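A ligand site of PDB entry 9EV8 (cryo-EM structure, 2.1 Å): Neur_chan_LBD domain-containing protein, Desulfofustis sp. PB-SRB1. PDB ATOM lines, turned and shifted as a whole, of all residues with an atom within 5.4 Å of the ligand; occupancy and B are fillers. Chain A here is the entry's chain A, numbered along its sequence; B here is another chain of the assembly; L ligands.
The side-chain sulfur of Cys 596 lies within hydrogen-bond range of an oxygen (O7) of the ligand (3.4 Å).
The guanidinium group (NE) of Arg 599 lies within salt-bridge range of an oxygen (O1) of the ligand (3.5 Å).
NE of Arg 599 sits at hydrogen-bond distance from O of Phe 538 of chain B (3.4 Å).
The side-chain hydroxyl (OG) of Ser 531 of chain B lies within hydrogen-bond range of the backbone carbonyl oxygen (O) of Phe 527 of chain B (2.9 Å).
Ile 593 touches the ligand (CD1 to C30, 3.9 Å).
Leu 600 touches the ligand.
CD1 of Ile 612 touches C25 of the ligand, at 3.9 Å.
Phe 527 of chain B touches the ligand (CE2 to C13, 3.9 Å).
CD2 of Leu 528 of chain B touches C15 of the ligand, 3.9 Å away.
OG of Ser 531 of chain B touches C13 of the ligand (3.6 Å).
Val 535 of chain B touches the ligand (CG2 to O6, 3.4 Å).
CD1 of Phe 538 of chain B touches C3 of the ligand, at 3.95 Å.
Within 4 Å of the ligand: Ile 593, Cys 596, Arg 599, Leu 600, Ile 612, Phe 527 of chain B, Leu 528 of chain B, Ser 531 of chain B, Val 535 of chain B and Phe 538 of chain B.
The nearest printed residue that does not touch the ligand is Trp 534 of chain B (4.03 Å).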
ATOM      1  N   LEU A 586      26.319 -11.436  -0.291  1.00  0.00           N
ATOM      2  CA  LEU A 586      27.320 -11.049  -1.279  1.00  0.00           C
ATOM      3  C   LEU A 586      28.008 -12.278  -1.871  1.00  0.00           C
ATOM      4  O   LEU A 586      28.283 -12.328  -3.090  1.00  0.00           O
ATOM      5  CB  LEU A 586      28.325 -10.091  -0.655  1.00  0.00           C
ATOM      6  CG  LEU A 586      27.727  -8.734  -0.301  1.00  0.00           C
ATOM      7  CD1 LEU A 586      28.745  -7.813   0.341  1.00  0.00           C
ATOM      8  CD2 LEU A 586      27.116  -8.073  -1.527  1.00  0.00           C
ATOM      9  N   ILE A 589      25.701 -13.675  -4.472  1.00  0.00           N
ATOM     10  CA  ILE A 589      25.658 -12.808  -5.646  1.00  0.00           C
ATOM     11  C   ILE A 589      26.901 -13.012  -6.505  1.00  0.00           C
ATOM     12  O   ILE A 589      26.836 -12.890  -7.737  1.00  0.00           O
ATOM     13  CB  ILE A 589      25.485 -11.338  -5.215  1.00  0.00           C
ATOM     14  CG1 ILE A 589      24.110 -11.138  -4.575  1.00  0.00           C
ATOM     15  CG2 ILE A 589      25.650 -10.389  -6.390  1.00  0.00           C
ATOM     16  CD1 ILE A 589      23.854  -9.729  -4.097  1.00  0.00           C
ATOM     17  N   LEU A 592      26.067 -15.865  -8.773  1.00  0.00           N
ATOM     18  CA  LEU A 592      25.155 -15.439  -9.835  1.00  0.00           C
ATOM     19  C   LEU A 592      25.894 -14.676 -10.943  1.00  0.00           C
ATOM     20  O   LEU A 592      25.685 -14.933 -12.141  1.00  0.00           O
ATOM     21  CB  LEU A 592      24.031 -14.577  -9.254  1.00  0.00           C
ATOM     22  CG  LEU A 592      23.069 -15.258  -8.284  1.00  0.00           C
ATOM     23  CD1 LEU A 592      22.061 -14.261  -7.738  1.00  0.00           C
ATOM     24  CD2 LEU A 592      22.350 -16.418  -8.956  1.00  0.00           C
ATOM     25  N   ILE A 593      26.764 -13.741 -10.548  1.00  0.00           N
ATOM     26  CA  ILE A 593      27.524 -12.974 -11.531  1.00  0.00           C
ATOM     27  C   ILE A 593      28.450 -13.872 -12.334  1.00  0.00           C
ATOM     28  O   ILE A 593      28.646 -13.677 -13.536  1.00  0.00           O
ATOM     29  CB  ILE A 593      28.292 -11.832 -10.829  1.00  0.00           C
ATOM     30  CG1 ILE A 593      27.330 -10.860 -10.159  1.00  0.00           C
ATOM     31  CG2 ILE A 593      29.170 -11.091 -11.821  1.00  0.00           C
ATOM     32  CD1 ILE A 593      28.013  -9.772  -9.369  1.00  0.00           C
ATOM     33  N   CYS A 596      26.435 -15.540 -15.032  1.00  0.00           N
ATOM     34  CA  CYS A 596      26.161 -14.588 -16.113  1.00  0.00           C
ATOM     35  C   CYS A 596      27.387 -14.375 -16.991  1.00  0.00           C
ATOM     36  O   CYS A 596      27.283 -14.336 -18.224  1.00  0.00           O
ATOM     37  CB  CYS A 596      25.667 -13.261 -15.528  1.00  0.00           C
ATOM     38  SG  CYS A 596      25.289 -12.010 -16.773  1.00  0.00           S
ATOM     39  N   ARG A 599      27.961 -17.330 -19.304  1.00  0.00           N
ATOM     40  CA  ARG A 599      27.075 -17.293 -20.462  1.00  0.00           C
ATOM     41  C   ARG A 599      27.538 -16.252 -21.478  1.00  0.00           C
ATOM     42  O   ARG A 599      27.560 -16.516 -22.697  1.00  0.00           O
ATOM     43  CB  ARG A 599      25.631 -17.033 -20.031  1.00  0.00           C
ATOM     44  CG  ARG A 599      24.638 -17.090 -21.171  1.00  0.00           C
ATOM     45  CD  ARG A 599      24.822 -18.364 -21.988  1.00  0.00           C
ATOM     46  NE  ARG A 599      24.051 -18.336 -23.220  1.00  0.00           N
ATOM     47  CZ  ARG A 599      24.186 -19.223 -24.207  1.00  0.00           C
ATOM     48  NH1 ARG A 599      25.048 -20.215 -24.125  1.00  0.00           N
ATOM     49  NH2 ARG A 599      23.426 -19.095 -25.290  1.00  0.00           N
ATOM     50  N   LEU A 600      27.924 -15.066 -21.002  1.00  0.00           N
ATOM     51  CA  LEU A 600      28.382 -14.021 -21.913  1.00  0.00           C
ATOM     52  C   LEU A 600      29.613 -14.469 -22.694  1.00  0.00           C
ATOM     53  O   LEU A 600      29.719 -14.214 -23.899  1.00  0.00           O
ATOM     54  CB  LEU A 600      28.689 -12.740 -21.140  1.00  0.00           C
ATOM     55  CG  LEU A 600      27.522 -11.811 -20.831  1.00  0.00           C
ATOM     56  CD1 LEU A 600      27.990 -10.627 -20.006  1.00  0.00           C
ATOM     57  CD2 LEU A 600      26.880 -11.335 -22.116  1.00  0.00           C
ATOM     58  N   VAL A 603      28.522 -16.852 -25.487  1.00  0.00           N
ATOM     59  CA  VAL A 603      27.908 -16.237 -26.660  1.00  0.00           C
ATOM     60  C   VAL A 603      28.886 -15.385 -27.459  1.00  0.00           C
ATOM     61  O   VAL A 603      28.569 -14.962 -28.581  1.00  0.00           O
ATOM     62  CB  VAL A 603      26.682 -15.414 -26.231  1.00  0.00           C
ATOM     63  CG1 VAL A 603      25.840 -14.999 -27.428  1.00  0.00           C
ATOM     64  CG2 VAL A 603      25.829 -16.203 -25.261  1.00  0.00           C
ATOM     65  N   ILE A 612      32.765  -6.293 -16.650  1.00  0.00           N
ATOM     66  CA  ILE A 612      32.087  -6.676 -15.415  1.00  0.00           C
ATOM     67  C   ILE A 612      33.098  -7.070 -14.349  1.00  0.00           C
ATOM     68  O   ILE A 612      32.936  -6.759 -13.162  1.00  0.00           O
ATOM     69  CB  ILE A 612      31.070  -7.806 -15.687  1.00  0.00           C
ATOM     70  CG1 ILE A 612      29.927  -7.301 -16.571  1.00  0.00           C
ATOM     71  CG2 ILE A 612      30.522  -8.361 -14.389  1.00  0.00           C
ATOM     72  CD1 ILE A 612      28.917  -8.374 -16.927  1.00  0.00           C
ATOM     73  N   TRP A 615      34.537  -3.909 -12.893  1.00  0.00           N
ATOM     74  CA  TRP A 615      33.545  -3.257 -12.052  1.00  0.00           C
ATOM     75  C   TRP A 615      33.402  -3.944 -10.697  1.00  0.00           C
ATOM     76  O   TRP A 615      33.362  -3.280  -9.657  1.00  0.00           O
ATOM     77  CB  TRP A 615      32.189  -3.214 -12.765  1.00  0.00           C
ATOM     78  CG  TRP A 615      32.085  -2.199 -13.849  1.00  0.00           C
ATOM     79  CD1 TRP A 615      32.982  -1.207 -14.128  1.00  0.00           C
ATOM     80  CD2 TRP A 615      31.029  -2.063 -14.795  1.00  0.00           C
ATOM     81  NE1 TRP A 615      32.542  -0.465 -15.199  1.00  0.00           N
ATOM     82  CE2 TRP A 615      31.339  -0.967 -15.623  1.00  0.00           C
ATOM     83  CE3 TRP A 615      29.841  -2.764 -15.026  1.00  0.00           C
ATOM     84  CZ2 TRP A 615      30.514  -0.560 -16.664  1.00  0.00           C
ATOM     85  CZ3 TRP A 615      29.013  -2.356 -16.058  1.00  0.00           C
ATOM     86  CH2 TRP A 615      29.357  -1.263 -16.863  1.00  0.00           C
ATOM     87  N   VAL A 616      33.323  -5.275 -10.692  1.00  0.00           N
ATOM     88  CA  VAL A 616      33.182  -6.006  -9.441  1.00  0.00           C
ATOM     89  C   VAL A 616      34.397  -5.809  -8.554  1.00  0.00           C
ATOM     90  O   VAL A 616      34.270  -5.532  -7.342  1.00  0.00           O
ATOM     91  CB  VAL A 616      32.919  -7.499  -9.723  1.00  0.00           C
ATOM     92  CG1 VAL A 616      33.009  -8.315  -8.448  1.00  0.00           C
ATOM     93  CG2 VAL A 616      31.560  -7.692 -10.375  1.00  0.00           C
ATOM     94  N   ILE A 619      34.141  -2.439  -7.001  1.00  0.00           N
ATOM     95  CA  ILE A 619      32.965  -2.082  -6.209  1.00  0.00           C
ATOM     96  C   ILE A 619      32.934  -2.824  -4.874  1.00  0.00           C
ATOM     97  O   ILE A 619      32.628  -2.223  -3.844  1.00  0.00           O
ATOM     98  CB  ILE A 619      31.680  -2.316  -7.035  1.00  0.00           C
ATOM     99  CG1 ILE A 619      31.456  -1.167  -8.007  1.00  0.00           C
ATOM    100  CG2 ILE A 619      30.480  -2.486  -6.126  1.00  0.00           C
ATOM    101  CD1 ILE A 619      30.237  -1.332  -8.886  1.00  0.00           C
ATOM    102  N   TYR A 620      33.107  -4.138  -4.895  1.00  0.00           N
ATOM    103  CA  TYR A 620      32.921  -4.948  -3.658  1.00  0.00           C
ATOM    104  C   TYR A 620      33.558  -4.448  -2.332  1.00  0.00           C
ATOM    105  O   TYR A 620      32.854  -4.373  -1.324  1.00  0.00           O
ATOM    106  CB  TYR A 620      33.297  -6.422  -3.918  1.00  0.00           C
ATOM    107  CG  TYR A 620      32.082  -7.309  -4.100  1.00  0.00           C
ATOM    108  CD1 TYR A 620      31.216  -7.117  -5.170  1.00  0.00           C
ATOM    109  CD2 TYR A 620      31.796  -8.313  -3.191  1.00  0.00           C
ATOM    110  CE1 TYR A 620      30.095  -7.918  -5.342  1.00  0.00           C
ATOM    111  CE2 TYR A 620      30.681  -9.117  -3.350  1.00  0.00           C
ATOM    112  CZ  TYR A 620      29.833  -8.910  -4.425  1.00  0.00           C
ATOM    113  OH  TYR A 620      28.729  -9.717  -4.590  1.00  0.00           O
ATOM    114  N   VAL A 623      31.621  -1.473  -1.063  1.00  0.00           N
ATOM    115  CA  VAL A 623      30.359  -1.843  -0.438  1.00  0.00           C
ATOM    116  C   VAL A 623      30.587  -2.325   0.984  1.00  0.00           C
ATOM    117  O   VAL A 623      29.857  -1.952   1.918  1.00  0.00           O
ATOM    118  CB  VAL A 623      29.630  -2.900  -1.288  1.00  0.00           C
ATOM    119  CG1 VAL A 623      28.361  -3.369  -0.587  1.00  0.00           C
ATOM    120  CG2 VAL A 623      29.294  -2.346  -2.655  1.00  0.00           C
ATOM    121  N   PHE B 527      16.081 -17.352  -0.750  1.00  0.00           N
ATOM    122  CA  PHE B 527      15.757 -16.795  -2.059  1.00  0.00           C
ATOM    123  C   PHE B 527      16.979 -16.758  -2.966  1.00  0.00           C
ATOM    124  O   PHE B 527      16.878 -17.081  -4.154  1.00  0.00           O
ATOM    125  CB  PHE B 527      15.168 -15.394  -1.896  1.00  0.00           C
ATOM    126  CG  PHE B 527      14.889 -14.695  -3.193  1.00  0.00           C
ATOM    127  CD1 PHE B 527      13.761 -15.005  -3.938  1.00  0.00           C
ATOM    128  CD2 PHE B 527      15.762 -13.731  -3.672  1.00  0.00           C
ATOM    129  CE1 PHE B 527      13.513 -14.366  -5.137  1.00  0.00           C
ATOM    130  CE2 PHE B 527      15.515 -13.093  -4.871  1.00  0.00           C
ATOM    131  CZ  PHE B 527      14.389 -13.415  -5.604  1.00  0.00           C
ATOM    132  N   LEU B 528      18.138 -16.366  -2.436  1.00  0.00           N
ATOM    133  CA  LEU B 528      19.352 -16.344  -3.249  1.00  0.00           C
ATOM    134  C   LEU B 528      19.746 -17.755  -3.708  1.00  0.00           C
ATOM    135  O   LEU B 528      20.175 -17.954  -4.844  1.00  0.00           O
ATOM    136  CB  LEU B 528      20.485 -15.670  -2.483  1.00  0.00           C
ATOM    137  CG  LEU B 528      20.302 -14.166  -2.291  1.00  0.00           C
ATOM    138  CD1 LEU B 528      21.427 -13.578  -1.461  1.00  0.00           C
ATOM    139  CD2 LEU B 528      20.209 -13.460  -3.627  1.00  0.00           C
ATOM    140  N   SER B 531      17.504 -18.717  -6.470  1.00  0.00           N
ATOM    141  CA  SER B 531      17.876 -17.978  -7.669  1.00  0.00           C
ATOM    142  C   SER B 531      19.093 -18.598  -8.363  1.00  0.00           C
ATOM    143  O   SER B 531      19.176 -18.565  -9.592  1.00  0.00           O
ATOM    144  CB  SER B 531      18.147 -16.515  -7.319  1.00  0.00           C
ATOM    145  OG  SER B 531      16.994 -15.903  -6.772  1.00  0.00           O
ATOM    146  N   TRP B 534      17.852 -21.344 -10.379  1.00  0.00           N
ATOM    147  CA  TRP B 534      17.046 -20.872 -11.501  1.00  0.00           C
ATOM    148  C   TRP B 534      17.886 -20.307 -12.640  1.00  0.00           C
ATOM    149  O   TRP B 534      17.576 -20.534 -13.811  1.00  0.00           O
ATOM    150  CB  TRP B 534      16.053 -19.801 -11.016  1.00  0.00           C
ATOM    151  CG  TRP B 534      15.270 -19.181 -12.123  1.00  0.00           C
ATOM    152  CD1 TRP B 534      14.204 -19.728 -12.773  1.00  0.00           C
ATOM    153  CD2 TRP B 534      15.475 -17.893 -12.709  1.00  0.00           C
ATOM    154  NE1 TRP B 534      13.740 -18.863 -13.729  1.00  0.00           N
ATOM    155  CE2 TRP B 534      14.497 -17.725 -13.712  1.00  0.00           C
ATOM    156  CE3 TRP B 534      16.389 -16.853 -12.482  1.00  0.00           C
ATOM    157  CZ2 TRP B 534      14.412 -16.573 -14.485  1.00  0.00           C
ATOM    158  CZ3 TRP B 534      16.309 -15.714 -13.253  1.00  0.00           C
ATOM    159  CH2 TRP B 534      15.325 -15.586 -14.247  1.00  0.00           C
ATOM    160  N   VAL B 535      18.958 -19.587 -12.323  1.00  0.00           N
ATOM    161  CA  VAL B 535      19.675 -18.824 -13.343  1.00  0.00           C
ATOM    162  C   VAL B 535      20.463 -19.729 -14.292  1.00  0.00           C
ATOM    163  O   VAL B 535      20.741 -19.355 -15.428  1.00  0.00           O
ATOM    164  CB  VAL B 535      20.584 -17.776 -12.682  1.00  0.00           C
ATOM    165  CG1 VAL B 535      21.782 -18.427 -12.018  1.00  0.00           C
ATOM    166  CG2 VAL B 535      21.034 -16.730 -13.692  1.00  0.00           C
ATOM    167  N   PHE B 538      20.023 -20.584 -18.336  1.00  0.00           N
ATOM    168  CA  PHE B 538      20.432 -19.787 -19.491  1.00  0.00           C
ATOM    169  C   PHE B 538      21.641 -20.382 -20.200  1.00  0.00           C
ATOM    170  O   PHE B 538      21.849 -20.108 -21.391  1.00  0.00           O
ATOM    171  CB  PHE B 538      20.730 -18.350 -19.057  1.00  0.00           C
ATOM    172  CG  PHE B 538      19.510 -17.528 -18.764  1.00  0.00           C
ATOM    173  CD1 PHE B 538      18.778 -16.972 -19.797  1.00  0.00           C
ATOM    174  CD2 PHE B 538      19.092 -17.314 -17.465  1.00  0.00           C
ATOM    175  CE1 PHE B 538      17.650 -16.208 -19.533  1.00  0.00           C
ATOM    176  CE2 PHE B 538      17.972 -16.554 -17.197  1.00  0.00           C
ATOM    177  CZ  PHE B 538      17.247 -16.010 -18.227  1.00  0.00           C
HETATM  178  O1  LIG L   1      21.576 -15.866 -23.603  1.00  0.00           O
HETATM  179  O2  LIG L   1      22.441 -13.585 -24.342  1.00  0.00           O
HETATM  180  P1  LIG L   1      21.316 -14.388 -23.705  1.00  0.00           P
HETATM  181  O3  LIG L   1      19.932 -14.029 -24.203  1.00  0.00           O
HETATM  182  O4  LIG L   1      21.302 -13.868 -22.182  1.00  0.00           O
HETATM  183  C1  LIG L   1      22.482 -13.331 -21.575  1.00  0.00           C
HETATM  184  C2  LIG L   1      22.151 -12.936 -20.132  1.00  0.00           C
HETATM  185  C3  LIG L   1      21.506 -14.136 -19.434  1.00  0.00           C
HETATM  186  O5  LIG L   1      21.982 -14.392 -18.132  1.00  0.00           O
HETATM  187  C4  LIG L   1      21.268 -13.939 -16.959  1.00  0.00           C
HETATM  188  O6  LIG L   1      21.756 -14.212 -15.887  1.00  0.00           O
HETATM  189  C5  LIG L   1      19.995 -13.132 -17.048  1.00  0.00           C
HETATM  190  C6  LIG L   1      19.949 -12.084 -15.938  1.00  0.00           C
HETATM  191  C7  LIG L   1      18.966 -12.486 -14.836  1.00  0.00           C
HETATM  192  C8  LIG L   1      19.647 -12.601 -13.474  1.00  0.00           C
HETATM  193  C9  LIG L   1      18.612 -12.537 -12.343  1.00  0.00           C
HETATM  194  C10 LIG L   1      19.205 -12.909 -10.983  1.00  0.00           C
HETATM  195  C11 LIG L   1      18.242 -13.708 -10.116  1.00  0.00           C
HETATM  196  C12 LIG L   1      17.394 -12.866  -9.187  1.00  0.00           C
HETATM  197  C13 LIG L   1      18.048 -12.668  -7.824  1.00  0.00           C
HETATM  198  C14 LIG L   1      18.449 -11.208  -7.672  1.00  0.00           C
HETATM  199  C15 LIG L   1      18.908 -10.869  -6.258  1.00  0.00           C
HETATM  200  C16 LIG L   1      20.247 -10.156  -6.238  1.00  0.00           C
HETATM  201  C17 LIG L   1      20.168  -8.785  -6.887  1.00  0.00           C
HETATM  202  C18 LIG L   1      20.248  -7.687  -5.829  1.00  0.00           C
HETATM  203  O7  LIG L   1      23.358 -12.482 -19.523  1.00  0.00           O
HETATM  204  C19 LIG L   1      23.457 -11.033 -19.620  1.00  0.00           C
HETATM  205  O8  LIG L   1      24.299 -10.564 -20.350  1.00  0.00           O
HETATM  206  C20 LIG L   1      22.573 -10.094 -18.835  1.00  0.00           C
HETATM  207  C21 LIG L   1      23.391  -8.887 -18.351  1.00  0.00           C
HETATM  208  C22 LIG L   1      23.233  -8.677 -16.850  1.00  0.00           C
HETATM  209  C23 LIG L   1      24.418  -7.944 -16.226  1.00  0.00           C
HETATM  210  C24 LIG L   1      24.722  -8.440 -14.809  1.00  0.00           C
HETATM  211  C25 LIG L   1      26.076  -7.917 -14.318  1.00  0.00           C
HETATM  212  C26 LIG L   1      25.908  -6.768 -13.331  1.00  0.00           C
HETATM  213  C27 LIG L   1      27.235  -6.158 -12.897  1.00  0.00           C
HETATM  214  C28 LIG L   1      26.994  -5.108 -11.837  1.00  0.00           C
HETATM  215  C29 LIG L   1      28.165  -4.943 -10.891  1.00  0.00           C
HETATM  216  C30 LIG L   1      28.014  -5.856  -9.690  1.00  0.00           C
HETATM  217  C31 LIG L   1      26.938  -5.367  -8.716  1.00  0.00           C
HETATM  218  C32 LIG L   1      27.370  -5.590  -7.271  1.00  0.00           C
HETATM  219  C33 LIG L   1      26.152  -5.754  -6.370  1.00  0.00           C
HETATM  220  C34 LIG L   1      26.560  -5.876  -4.916  1.00  0.00           C
